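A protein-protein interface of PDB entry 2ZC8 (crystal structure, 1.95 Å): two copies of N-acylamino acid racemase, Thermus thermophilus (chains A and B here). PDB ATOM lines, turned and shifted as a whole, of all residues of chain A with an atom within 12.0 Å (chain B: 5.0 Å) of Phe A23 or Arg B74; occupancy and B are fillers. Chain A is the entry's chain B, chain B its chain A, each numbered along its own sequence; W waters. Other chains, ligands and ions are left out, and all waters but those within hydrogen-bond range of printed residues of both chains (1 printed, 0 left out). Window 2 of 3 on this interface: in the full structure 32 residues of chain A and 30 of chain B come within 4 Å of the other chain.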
ATOM      1  N   ARG A  18      -3.942 -26.512  16.366  1.00  0.00           N
ATOM      2  CA  ARG A  18      -4.007 -26.684  14.919  1.00  0.00           C
ATOM      3  C   ARG A  18      -4.039 -25.273  14.331  1.00  0.00           C
ATOM      4  O   ARG A  18      -4.821 -24.437  14.765  1.00  0.00           O
ATOM      5  CB  ARG A  18      -5.279 -27.465  14.544  1.00  0.00           C
ATOM      6  CG  ARG A  18      -5.338 -28.889  15.138  1.00  0.00           C
ATOM      7  CD  ARG A  18      -6.692 -29.599  14.824  1.00  0.00           C
ATOM      8  NE  ARG A  18      -6.939 -29.734  13.383  1.00  0.00           N
ATOM      9  CZ  ARG A  18      -6.321 -30.616  12.598  1.00  0.00           C
ATOM     10  NH1 ARG A  18      -5.427 -31.451  13.117  1.00  0.00           N
ATOM     11  NH2 ARG A  18      -6.578 -30.660  11.285  1.00  0.00           N
ATOM     12  N   PHE A  19      -3.177 -25.006  13.354  1.00  0.00           N
ATOM     13  CA  PHE A  19      -3.099 -23.668  12.760  1.00  0.00           C
ATOM     14  C   PHE A  19      -3.621 -23.658  11.330  1.00  0.00           C
ATOM     15  O   PHE A  19      -3.068 -24.312  10.452  1.00  0.00           O
ATOM     16  CB  PHE A  19      -1.643 -23.181  12.786  1.00  0.00           C
ATOM     17  CG  PHE A  19      -1.465 -21.787  12.262  1.00  0.00           C
ATOM     18  CD1 PHE A  19      -2.015 -20.698  12.941  1.00  0.00           C
ATOM     19  CD2 PHE A  19      -0.774 -21.560  11.081  1.00  0.00           C
ATOM     20  CE1 PHE A  19      -1.875 -19.394  12.436  1.00  0.00           C
ATOM     21  CE2 PHE A  19      -0.632 -20.269  10.571  1.00  0.00           C
ATOM     22  CZ  PHE A  19      -1.184 -19.187  11.252  1.00  0.00           C
ATOM     23  N   GLU A  20      -4.681 -22.903  11.088  1.00  0.00           N
ATOM     24  CA  GLU A  20      -5.258 -22.872   9.752  1.00  0.00           C
ATOM     25  C   GLU A  20      -4.431 -22.021   8.783  1.00  0.00           C
ATOM     26  O   GLU A  20      -3.988 -20.926   9.129  1.00  0.00           O
ATOM     27  CB  GLU A  20      -6.680 -22.341   9.817  1.00  0.00           C
ATOM     28  CG  GLU A  20      -7.522 -22.789   8.652  1.00  0.00           C
ATOM     29  CD  GLU A  20      -8.983 -22.469   8.860  1.00  0.00           C
ATOM     30  OE1 GLU A  20      -9.529 -22.855   9.927  1.00  0.00           O
ATOM     31  OE2 GLU A  20      -9.578 -21.837   7.961  1.00  0.00           O
ATOM     32  N   THR A  21      -4.221 -22.536   7.575  1.00  0.00           N
ATOM     33  CA  THR A  21      -3.459 -21.808   6.562  1.00  0.00           C
ATOM     34  C   THR A  21      -4.257 -21.850   5.269  1.00  0.00           C
ATOM     35  O   THR A  21      -5.364 -22.404   5.235  1.00  0.00           O
ATOM     36  CB  THR A  21      -2.106 -22.461   6.283  1.00  0.00           C
ATOM     37  OG1 THR A  21      -2.315 -23.636   5.494  1.00  0.00           O
ATOM     38  CG2 THR A  21      -1.393 -22.831   7.594  1.00  0.00           C
ATOM     39  N   SER A  22      -3.686 -21.296   4.199  1.00  0.00           N
ATOM     40  CA  SER A  22      -4.357 -21.268   2.896  1.00  0.00           C
ATOM     41  C   SER A  22      -4.248 -22.589   2.135  1.00  0.00           C
ATOM     42  O   SER A  22      -4.840 -22.756   1.070  1.00  0.00           O
ATOM     43  CB  SER A  22      -3.767 -20.145   2.044  1.00  0.00           C
ATOM     44  OG  SER A  22      -2.350 -20.284   1.960  1.00  0.00           O
ATOM     45  N   PHE A  23      -3.472 -23.522   2.659  1.00  0.00           N
ATOM     46  CA  PHE A  23      -3.330 -24.813   2.008  1.00  0.00           C
ATOM     47  C   PHE A  23      -3.080 -25.906   3.041  1.00  0.00           C
ATOM     48  O   PHE A  23      -1.984 -26.473   3.097  1.00  0.00           O
ATOM     49  CB  PHE A  23      -2.165 -24.810   1.028  1.00  0.00           C
ATOM     50  CG  PHE A  23      -2.171 -25.977   0.092  1.00  0.00           C
ATOM     51  CD1 PHE A  23      -3.114 -26.056  -0.925  1.00  0.00           C
ATOM     52  CD2 PHE A  23      -1.251 -27.007   0.237  1.00  0.00           C
ATOM     53  CE1 PHE A  23      -3.143 -27.159  -1.794  1.00  0.00           C
ATOM     54  CE2 PHE A  23      -1.268 -28.111  -0.621  1.00  0.00           C
ATOM     55  CZ  PHE A  23      -2.218 -28.187  -1.639  1.00  0.00           C
ATOM     56  N   GLY A  24      -4.102 -26.194   3.842  1.00  0.00           N
ATOM     57  CA  GLY A  24      -3.991 -27.209   4.868  1.00  0.00           C
ATOM     58  C   GLY A  24      -4.060 -26.633   6.274  1.00  0.00           C
ATOM     59  O   GLY A  24      -4.153 -25.407   6.484  1.00  0.00           O
ATOM     60  N   VAL A  25      -4.053 -27.530   7.252  1.00  0.00           N
ATOM     61  CA  VAL A  25      -4.069 -27.106   8.636  1.00  0.00           C
ATOM     62  C   VAL A  25      -2.713 -27.572   9.121  1.00  0.00           C
ATOM     63  O   VAL A  25      -2.343 -28.741   8.937  1.00  0.00           O
ATOM     64  CB  VAL A  25      -5.208 -27.766   9.437  1.00  0.00           C
ATOM     65  CG1 VAL A  25      -5.036 -27.458  10.934  1.00  0.00           C
ATOM     66  CG2 VAL A  25      -6.558 -27.239   8.935  1.00  0.00           C
ATOM     67  N   GLN A  26      -1.968 -26.642   9.702  1.00  0.00           N
ATOM     68  CA  GLN A  26      -0.617 -26.910  10.180  1.00  0.00           C
ATOM     69  C   GLN A  26      -0.609 -27.373  11.629  1.00  0.00           C
ATOM     70  O   GLN A  26      -1.294 -26.788  12.488  1.00  0.00           O
ATOM     71  CB  GLN A  26       0.230 -25.634  10.016  1.00  0.00           C
ATOM     72  CG  GLN A  26       1.722 -25.789  10.247  1.00  0.00           C
ATOM     73  CD  GLN A  26       2.431 -24.441  10.208  1.00  0.00           C
ATOM     74  OE1 GLN A  26       1.899 -23.470   9.665  1.00  0.00           O
ATOM     75  NE2 GLN A  26       3.620 -24.374  10.780  1.00  0.00           N
ATOM     76  N   THR A  27       0.178 -28.414  11.902  1.00  0.00           N
ATOM     77  CA  THR A  27       0.282 -28.973  13.261  1.00  0.00           C
ATOM     78  C   THR A  27       1.726 -29.057  13.755  1.00  0.00           C
ATOM     79  O   THR A  27       1.980 -29.454  14.902  1.00  0.00           O
ATOM     80  CB  THR A  27      -0.289 -30.398  13.317  1.00  0.00           C
ATOM     81  OG1 THR A  27       0.506 -31.233  12.465  1.00  0.00           O
ATOM     82  CG2 THR A  27      -1.761 -30.406  12.875  1.00  0.00           C
ATOM     83  N   LYS A  28       2.666 -28.688  12.892  1.00  0.00           N
ATOM     84  CA  LYS A  28       4.082 -28.720  13.231  1.00  0.00           C
ATOM     85  C   LYS A  28       4.799 -27.533  12.598  1.00  0.00           C
ATOM     86  O   LYS A  28       4.317 -26.979  11.600  1.00  0.00           O
ATOM     87  CB  LYS A  28       4.697 -30.024  12.713  1.00  0.00           C
ATOM     88  CG  LYS A  28       4.047 -31.240  13.395  1.00  0.00           C
ATOM     89  CD  LYS A  28       4.299 -32.561  12.701  1.00  0.00           C
ATOM     90  CE  LYS A  28       3.584 -33.676  13.483  1.00  0.00           C
ATOM     91  NZ  LYS A  28       3.671 -35.021  12.844  1.00  0.00           N
ATOM     92  N   GLU A  50       8.437 -21.532   6.164  1.00  0.00           N
ATOM     93  CA  GLU A  50       7.900 -22.870   6.342  1.00  0.00           C
ATOM     94  C   GLU A  50       8.153 -23.777   5.143  1.00  0.00           C
ATOM     95  O   GLU A  50       8.863 -23.401   4.196  1.00  0.00           O
ATOM     96  CB  GLU A  50       6.402 -22.757   6.607  1.00  0.00           C
ATOM     97  CG  GLU A  50       6.079 -22.949   8.077  1.00  0.00           C
ATOM     98  CD  GLU A  50       6.406 -24.387   8.545  1.00  0.00           C
ATOM     99  OE1 GLU A  50       6.770 -24.557   9.722  1.00  0.00           O
ATOM    100  OE2 GLU A  50       6.294 -25.323   7.716  1.00  0.00           O
ATOM    101  N   ARG A  51       7.577 -24.981   5.173  1.00  0.00           N
ATOM    102  CA  ARG A  51       7.767 -25.909   4.060  1.00  0.00           C
ATOM    103  C   ARG A  51       7.068 -25.447   2.782  1.00  0.00           C
ATOM    104  O   ARG A  51       7.532 -25.749   1.678  1.00  0.00           O
ATOM    105  CB  ARG A  51       7.231 -27.302   4.410  1.00  0.00           C
ATOM    106  CG  ARG A  51       8.014 -27.988   5.499  1.00  0.00           C
ATOM    107  CD  ARG A  51       7.328 -29.290   5.904  1.00  0.00           C
ATOM    108  NE  ARG A  51       8.221 -30.083   6.738  1.00  0.00           N
ATOM    109  CZ  ARG A  51       8.980 -31.075   6.284  1.00  0.00           C
ATOM    110  NH1 ARG A  51       8.948 -31.412   4.994  1.00  0.00           N
ATOM    111  NH2 ARG A  51       9.789 -31.714   7.122  1.00  0.00           N
ATOM    112  N   LEU A  52       5.936 -24.772   2.948  1.00  0.00           N
ATOM    113  CA  LEU A  52       5.164 -24.264   1.808  1.00  0.00           C
ATOM    114  C   LEU A  52       5.158 -22.719   1.813  1.00  0.00           C
ATOM    115  O   LEU A  52       5.077 -22.108   2.891  1.00  0.00           O
ATOM    116  CB  LEU A  52       3.725 -24.766   1.907  1.00  0.00           C
ATOM    117  CG  LEU A  52       3.605 -26.296   1.970  1.00  0.00           C
ATOM    118  CD1 LEU A  52       2.161 -26.697   2.271  1.00  0.00           C
ATOM    119  CD2 LEU A  52       4.067 -26.885   0.653  1.00  0.00           C
ATOM    120  N   PRO A  53       5.222 -22.083   0.619  1.00  0.00           N
ATOM    121  CA  PRO A  53       5.222 -20.612   0.520  1.00  0.00           C
ATOM    122  C   PRO A  53       3.802 -20.058   0.650  1.00  0.00           C
ATOM    123  O   PRO A  53       3.220 -19.597  -0.331  1.00  0.00           O
ATOM    124  CB  PRO A  53       5.812 -20.370  -0.873  1.00  0.00           C
ATOM    125  CG  PRO A  53       5.224 -21.514  -1.677  1.00  0.00           C
ATOM    126  CD  PRO A  53       5.439 -22.699  -0.716  1.00  0.00           C
ATOM    127  N   LEU A  54       3.240 -20.107   1.861  1.00  0.00           N
ATOM    128  CA  LEU A  54       1.850 -19.685   2.061  1.00  0.00           C
ATOM    129  C   LEU A  54       1.742 -18.272   2.598  1.00  0.00           C
ATOM    130  O   LEU A  54       0.956 -17.477   2.094  1.00  0.00           O
ATOM    131  CB  LEU A  54       1.140 -20.677   3.008  1.00  0.00           C
ATOM    132  CG  LEU A  54       1.142 -22.116   2.451  1.00  0.00           C
ATOM    133  CD1 LEU A  54       0.482 -23.055   3.480  1.00  0.00           C
ATOM    134  CD2 LEU A  54       0.369 -22.183   1.124  1.00  0.00           C
ATOM    135  N   TYR A  55       2.536 -17.960   3.612  1.00  0.00           N
ATOM    136  CA  TYR A  55       2.542 -16.597   4.162  1.00  0.00           C
ATOM    137  C   TYR A  55       3.257 -15.703   3.115  1.00  0.00           C
ATOM    138  O   TYR A  55       2.781 -14.603   2.776  1.00  0.00           O
ATOM    139  CB  TYR A  55       3.288 -16.582   5.482  1.00  0.00           C
ATOM    140  CG  TYR A  55       3.617 -15.180   5.947  1.00  0.00           C
ATOM    141  CD1 TYR A  55       2.656 -14.372   6.598  1.00  0.00           C
ATOM    142  CD2 TYR A  55       4.881 -14.654   5.704  1.00  0.00           C
ATOM    143  CE1 TYR A  55       2.985 -13.053   6.994  1.00  0.00           C
ATOM    144  CE2 TYR A  55       5.217 -13.356   6.081  1.00  0.00           C
ATOM    145  CZ  TYR A  55       4.280 -12.562   6.723  1.00  0.00           C
ATOM    146  OH  TYR A  55       4.684 -11.297   7.104  1.00  0.00           O
ATOM    147  N   ARG A  56       4.402 -16.157   2.628  1.00  0.00           N
ATOM    148  CA  ARG A  56       5.127 -15.464   1.562  1.00  0.00           C
ATOM    149  C   ARG A  56       5.943 -16.478   0.720  1.00  0.00           C
ATOM    150  O   ARG A  56       5.796 -17.692   0.884  1.00  0.00           O
ATOM    151  CB  ARG A  56       5.984 -14.266   2.069  1.00  0.00           C
ATOM    152  CG  ARG A  56       5.363 -12.892   1.632  1.00  0.00           C
ATOM    153  CD  ARG A  56       6.209 -11.665   2.064  1.00  0.00           C
ATOM    154  NE  ARG A  56       5.651 -10.405   1.525  1.00  0.00           N
ATOM    155  CZ  ARG A  56       5.825 -10.001   0.264  1.00  0.00           C
ATOM    156  NH1 ARG A  56       6.546 -10.735  -0.594  1.00  0.00           N
ATOM    157  NH2 ARG A  56       5.273  -8.859  -0.157  1.00  0.00           N
ATOM    158  N   THR A  59      10.825 -20.742   1.286  1.00  0.00           N
ATOM    159  CA  THR A  59      10.602 -22.066   1.877  1.00  0.00           C
ATOM    160  C   THR A  59      11.838 -22.472   2.667  1.00  0.00           C
ATOM    161  O   THR A  59      12.916 -21.891   2.520  1.00  0.00           O
ATOM    162  CB  THR A  59      10.363 -23.204   0.823  1.00  0.00           C
ATOM    163  OG1 THR A  59      11.575 -23.431   0.096  1.00  0.00           O
ATOM    164  CG2 THR A  59       9.197 -22.835  -0.113  1.00  0.00           C
ATOM    165  N   LYS A 163      -9.653 -12.603  13.379  1.00  0.00           N
ATOM    166  CA  LYS A 163      -9.576 -12.830  11.940  1.00  0.00           C
ATOM    167  C   LYS A 163     -10.996 -12.588  11.362  1.00  0.00           C
ATOM    168  O   LYS A 163     -12.009 -12.930  11.981  1.00  0.00           O
ATOM    169  CB  LYS A 163      -9.107 -14.265  11.677  1.00  0.00           C
ATOM    170  CG  LYS A 163      -9.074 -14.684  10.219  1.00  0.00           C
ATOM    171  CD  LYS A 163      -8.213 -15.949  10.054  1.00  0.00           C
ATOM    172  CE  LYS A 163      -8.157 -16.425   8.601  1.00  0.00           C
ATOM    173  NZ  LYS A 163      -7.177 -17.555   8.409  1.00  0.00           N
ATOM    174  N   ASN A 190      -6.563 -10.606   6.670  1.00  0.00           N
ATOM    175  CA  ASN A 190      -5.973 -11.730   5.924  1.00  0.00           C
ATOM    176  C   ASN A 190      -5.899 -11.657   4.394  1.00  0.00           C
ATOM    177  O   ASN A 190      -6.049 -12.681   3.723  1.00  0.00           O
ATOM    178  CB  ASN A 190      -6.827 -12.945   6.354  1.00  0.00           C
ATOM    179  CG  ASN A 190      -6.173 -14.295   6.097  1.00  0.00           C
ATOM    180  OD1 ASN A 190      -6.882 -15.276   5.817  1.00  0.00           O
ATOM    181  ND2 ASN A 190      -4.847 -14.374   6.219  1.00  0.00           N
ATOM    182  N   VAL B  70       5.858 -29.799  -4.464  1.00  0.00           N
ATOM    183  CA  VAL B  70       4.625 -29.064  -4.254  1.00  0.00           C
ATOM    184  C   VAL B  70       3.749 -28.961  -5.503  1.00  0.00           C
ATOM    185  O   VAL B  70       2.593 -29.418  -5.498  1.00  0.00           O
ATOM    186  CB  VAL B  70       4.926 -27.605  -3.715  1.00  0.00           C
ATOM    187  CG1 VAL B  70       3.644 -26.901  -3.350  1.00  0.00           C
ATOM    188  CG2 VAL B  70       5.852 -27.662  -2.486  1.00  0.00           C
ATOM    189  N   PHE B  71       4.298 -28.381  -6.567  1.00  0.00           N
ATOM    190  CA  PHE B  71       3.534 -28.162  -7.806  1.00  0.00           C
ATOM    191  C   PHE B  71       3.198 -29.400  -8.627  1.00  0.00           C
ATOM    192  O   PHE B  71       2.046 -29.569  -9.036  1.00  0.00           O
ATOM    193  CB  PHE B  71       4.254 -27.144  -8.730  1.00  0.00           C
ATOM    194  CG  PHE B  71       4.576 -25.786  -8.064  1.00  0.00           C
ATOM    195  CD1 PHE B  71       5.483 -24.910  -8.678  1.00  0.00           C
ATOM    196  CD2 PHE B  71       3.956 -25.387  -6.874  1.00  0.00           C
ATOM    197  CE1 PHE B  71       5.773 -23.661  -8.137  1.00  0.00           C
ATOM    198  CE2 PHE B  71       4.228 -24.122  -6.297  1.00  0.00           C
ATOM    199  CZ  PHE B  71       5.138 -23.259  -6.931  1.00  0.00           C
ATOM    200  N   LEU B  72       4.175 -30.271  -8.886  1.00  0.00           N
ATOM    201  CA  LEU B  72       3.850 -31.449  -9.685  1.00  0.00           C
ATOM    202  C   LEU B  72       2.897 -32.356  -8.904  1.00  0.00           C
ATOM    203  O   LEU B  72       1.941 -32.882  -9.478  1.00  0.00           O
ATOM    204  CB  LEU B  72       5.121 -32.169 -10.168  1.00  0.00           C
ATOM    205  CG  LEU B  72       5.861 -31.336 -11.248  1.00  0.00           C
ATOM    206  CD1 LEU B  72       7.288 -31.871 -11.470  1.00  0.00           C
ATOM    207  CD2 LEU B  72       5.076 -31.315 -12.564  1.00  0.00           C
ATOM    208  N   PRO B  73       3.131 -32.546  -7.586  1.00  0.00           N
ATOM    209  CA  PRO B  73       2.187 -33.407  -6.854  1.00  0.00           C
ATOM    210  C   PRO B  73       0.777 -32.783  -6.871  1.00  0.00           C
ATOM    211  O   PRO B  73      -0.224 -33.489  -6.882  1.00  0.00           O
ATOM    212  CB  PRO B  73       2.777 -33.463  -5.446  1.00  0.00           C
ATOM    213  CG  PRO B  73       4.247 -33.402  -5.691  1.00  0.00           C
ATOM    214  CD  PRO B  73       4.383 -32.357  -6.819  1.00  0.00           C
ATOM    215  N   ARG B  74       0.706 -31.453  -6.912  1.00  0.00           N
ATOM    216  CA  ARG B  74      -0.581 -30.766  -6.937  1.00  0.00           C
ATOM    217  C   ARG B  74      -1.364 -31.000  -8.248  1.00  0.00           C
ATOM    218  O   ARG B  74      -2.596 -31.087  -8.239  1.00  0.00           O
ATOM    219  CB  ARG B  74      -0.350 -29.268  -6.714  1.00  0.00           C
ATOM    220  CG  ARG B  74      -1.578 -28.351  -6.726  1.00  0.00           C
ATOM    221  CD  ARG B  74      -2.504 -28.554  -5.537  1.00  0.00           C
ATOM    222  NE  ARG B  74      -3.533 -27.512  -5.483  1.00  0.00           N
ATOM    223  CZ  ARG B  74      -4.724 -27.685  -4.914  1.00  0.00           C
ATOM    224  NH1 ARG B  74      -5.018 -28.856  -4.361  1.00  0.00           N
ATOM    225  NH2 ARG B  74      -5.626 -26.705  -4.906  1.00  0.00           N
ATOM    226  N   VAL B  75      -0.660 -31.148  -9.364  1.00  0.00           N
ATOM    227  CA  VAL B  75      -1.349 -31.306 -10.643  1.00  0.00           C
ATOM    228  C   VAL B  75      -1.292 -32.678 -11.315  1.00  0.00           C
ATOM    229  O   VAL B  75      -2.067 -32.944 -12.260  1.00  0.00           O
ATOM    230  CB  VAL B  75      -0.858 -30.237 -11.660  1.00  0.00           C
ATOM    231  CG1 VAL B  75      -1.058 -28.823 -11.060  1.00  0.00           C
ATOM    232  CG2 VAL B  75       0.613 -30.493 -12.041  1.00  0.00           C
ATOM    233  N   LEU B  76      -0.397 -33.548 -10.849  1.00  0.00           N
ATOM    234  CA  LEU B  76      -0.301 -34.876 -11.451  1.00  0.00           C
ATOM    235  C   LEU B  76      -1.634 -35.615 -11.352  1.00  0.00           C
ATOM    236  O   LEU B  76      -2.243 -35.704 -10.269  1.00  0.00           O
ATOM    237  CB  LEU B  76       0.823 -35.698 -10.782  1.00  0.00           C
ATOM    238  CG  LEU B  76       2.220 -35.406 -11.350  1.00  0.00           C
ATOM    239  CD1 LEU B  76       3.289 -36.069 -10.480  1.00  0.00           C
ATOM    240  CD2 LEU B  76       2.310 -35.894 -12.793  1.00  0.00           C
ATOM    241  N   ARG B  78      -4.486 -34.710 -12.345  1.00  0.00           N
ATOM    242  CA  ARG B  78      -5.677 -33.865 -12.294  1.00  0.00           C
ATOM    243  C   ARG B  78      -6.175 -33.514 -13.702  1.00  0.00           C
ATOM    244  O   ARG B  78      -5.387 -33.395 -14.641  1.00  0.00           O
ATOM    245  CB  ARG B  78      -5.389 -32.593 -11.496  1.00  0.00           C
ATOM    246  CG  ARG B  78      -5.293 -32.823 -10.012  1.00  0.00           C
ATOM    247  CD  ARG B  78      -5.203 -31.502  -9.265  1.00  0.00           C
ATOM    248  NE  ARG B  78      -6.122 -30.513  -9.821  1.00  0.00           N
ATOM    249  CZ  ARG B  78      -6.278 -29.288  -9.338  1.00  0.00           C
ATOM    250  NH1 ARG B  78      -5.576 -28.897  -8.280  1.00  0.00           N
ATOM    251  NH2 ARG B  78      -7.128 -28.452  -9.924  1.00  0.00           N
ATOM    252  N   ALA B  89      -4.923 -24.069  -9.759  1.00  0.00           N
ATOM    253  CA  ALA B  89      -4.363 -25.134  -8.919  1.00  0.00           C
ATOM    254  C   ALA B  89      -3.134 -24.639  -8.085  1.00  0.00           C
ATOM    255  O   ALA B  89      -2.914 -25.081  -6.958  1.00  0.00           O
ATOM    256  CB  ALA B  89      -3.936 -26.338  -9.834  1.00  0.00           C
ATOM    257  N   LEU B  90      -2.347 -23.722  -8.646  1.00  0.00           N
ATOM    258  CA  LEU B  90      -1.130 -23.203  -7.986  1.00  0.00           C
ATOM    259  C   LEU B  90      -1.315 -21.907  -7.246  1.00  0.00           C
ATOM    260  O   LEU B  90      -0.368 -21.383  -6.665  1.00  0.00           O
ATOM    261  CB  LEU B  90      -0.024 -22.967  -9.035  1.00  0.00           C
ATOM    262  CG  LEU B  90       0.305 -24.216  -9.851  1.00  0.00           C
ATOM    263  CD1 LEU B  90       1.438 -23.913 -10.818  1.00  0.00           C
ATOM    264  CD2 LEU B  90       0.700 -25.332  -8.870  1.00  0.00           C
ATOM    265  N   PRO B  92      -2.628 -21.018  -4.367  1.00  0.00           N
ATOM    266  CA  PRO B  92      -2.348 -20.850  -2.937  1.00  0.00           C
ATOM    267  C   PRO B  92      -0.900 -20.505  -2.616  1.00  0.00           C
ATOM    268  O   PRO B  92      -0.617 -19.973  -1.543  1.00  0.00           O
ATOM    269  CB  PRO B  92      -2.723 -22.215  -2.350  1.00  0.00           C
ATOM    270  CG  PRO B  92      -3.716 -22.767  -3.362  1.00  0.00           C
ATOM    271  CD  PRO B  92      -3.078 -22.393  -4.655  1.00  0.00           C
ATOM    272  N   PHE B  93       0.005 -20.821  -3.545  1.00  0.00           N
ATOM    273  CA  PHE B  93       1.436 -20.609  -3.353  1.00  0.00           C
ATOM    274  C   PHE B  93       1.852 -19.228  -3.808  1.00  0.00           C
ATOM    275  O   PHE B  93       1.694 -18.899  -4.976  1.00  0.00           O
ATOM    276  CB  PHE B  93       2.186 -21.724  -4.093  1.00  0.00           C
ATOM    277  CG  PHE B  93       1.604 -23.098  -3.792  1.00  0.00           C
ATOM    278  CD1 PHE B  93       0.951 -23.825  -4.778  1.00  0.00           C
ATOM    279  CD2 PHE B  93       1.626 -23.595  -2.484  1.00  0.00           C
ATOM    280  CE1 PHE B  93       0.319 -25.025  -4.482  1.00  0.00           C
ATOM    281  CE2 PHE B  93       0.993 -24.802  -2.160  1.00  0.00           C
ATOM    282  CZ  PHE B  93       0.337 -25.515  -3.163  1.00  0.00           C
HETATM  283  O   HOH W   1      -1.231 -18.473   0.541  1.00  0.00           O
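Of chain B, only Arg B74 and Phe B93 come within 4 Å of Phe A23.
Printed residues of chain B within 4 Å of Leu A52: Val B70.
Of the printed residues of chain B, Pro A53 touches Phe B93.
Printed residues of chain B within 4 Å of Leu A54: Pro B92 (3.6 Å).
Of chain A, only Leu A52 (3.7 Å) comes within 4 Å of Val B70.
No residue of chain A comes within 4 Å of Pro B73.
Of chain A, only Phe A23 comes within 4 Å of Arg B74.
Val B75 touches none of the printed residues of chain A.
No residue of chain A comes within 4 Å of Arg B78.
No residue of chain A comes within 4 Å of Leu B90.
Printed residues of chain A within 4 Å of Phe B93: Phe A23 and Pro A53.
The nearest residue of chain B that does not touch Phe A23 is Pro B92 (4.1 Å).
The nearest residue of chain A that does not touch Arg B74 is Ser A22 (7.2 Å).
NE of Arg B74 lies within hydrogen-bond range of O of Ala B89, at 2.9 Å.
The side-chain hydroxyl of Thr A21 lies within hydrogen-bond range of the backbone NH of Phe A23 (3.1 Å).
Among the printed residues, merely in contact across the chains: Ser A22 with Pro B92, Phe A23 with Arg B74, Phe A23 with Phe B93, Leu A52 with Val B70, Pro A53 with Phe B93 and Leu A54 with Pro B92.
Water W1 lies within hydrogen-bond range of the side-chain hydroxyl (OG) of Ser A22, the backbone carbonyl oxygen (O) of Pro B92 and the backbone carbonyl oxygen (O) of Leu A54.
No position is printed for both chains.
Of the 6 pairs that touch across the chains among the printed residues, none has its exchanged pair printed and touching as well.
Of the 21 printed residues of chain A, 5 touch a printed residue of chain B.
Hydrophobic or aromatic side chains of chain A within 4 Å of the printed part of chain B: Phe A23, Leu A52, Pro A53 and Leu A54.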
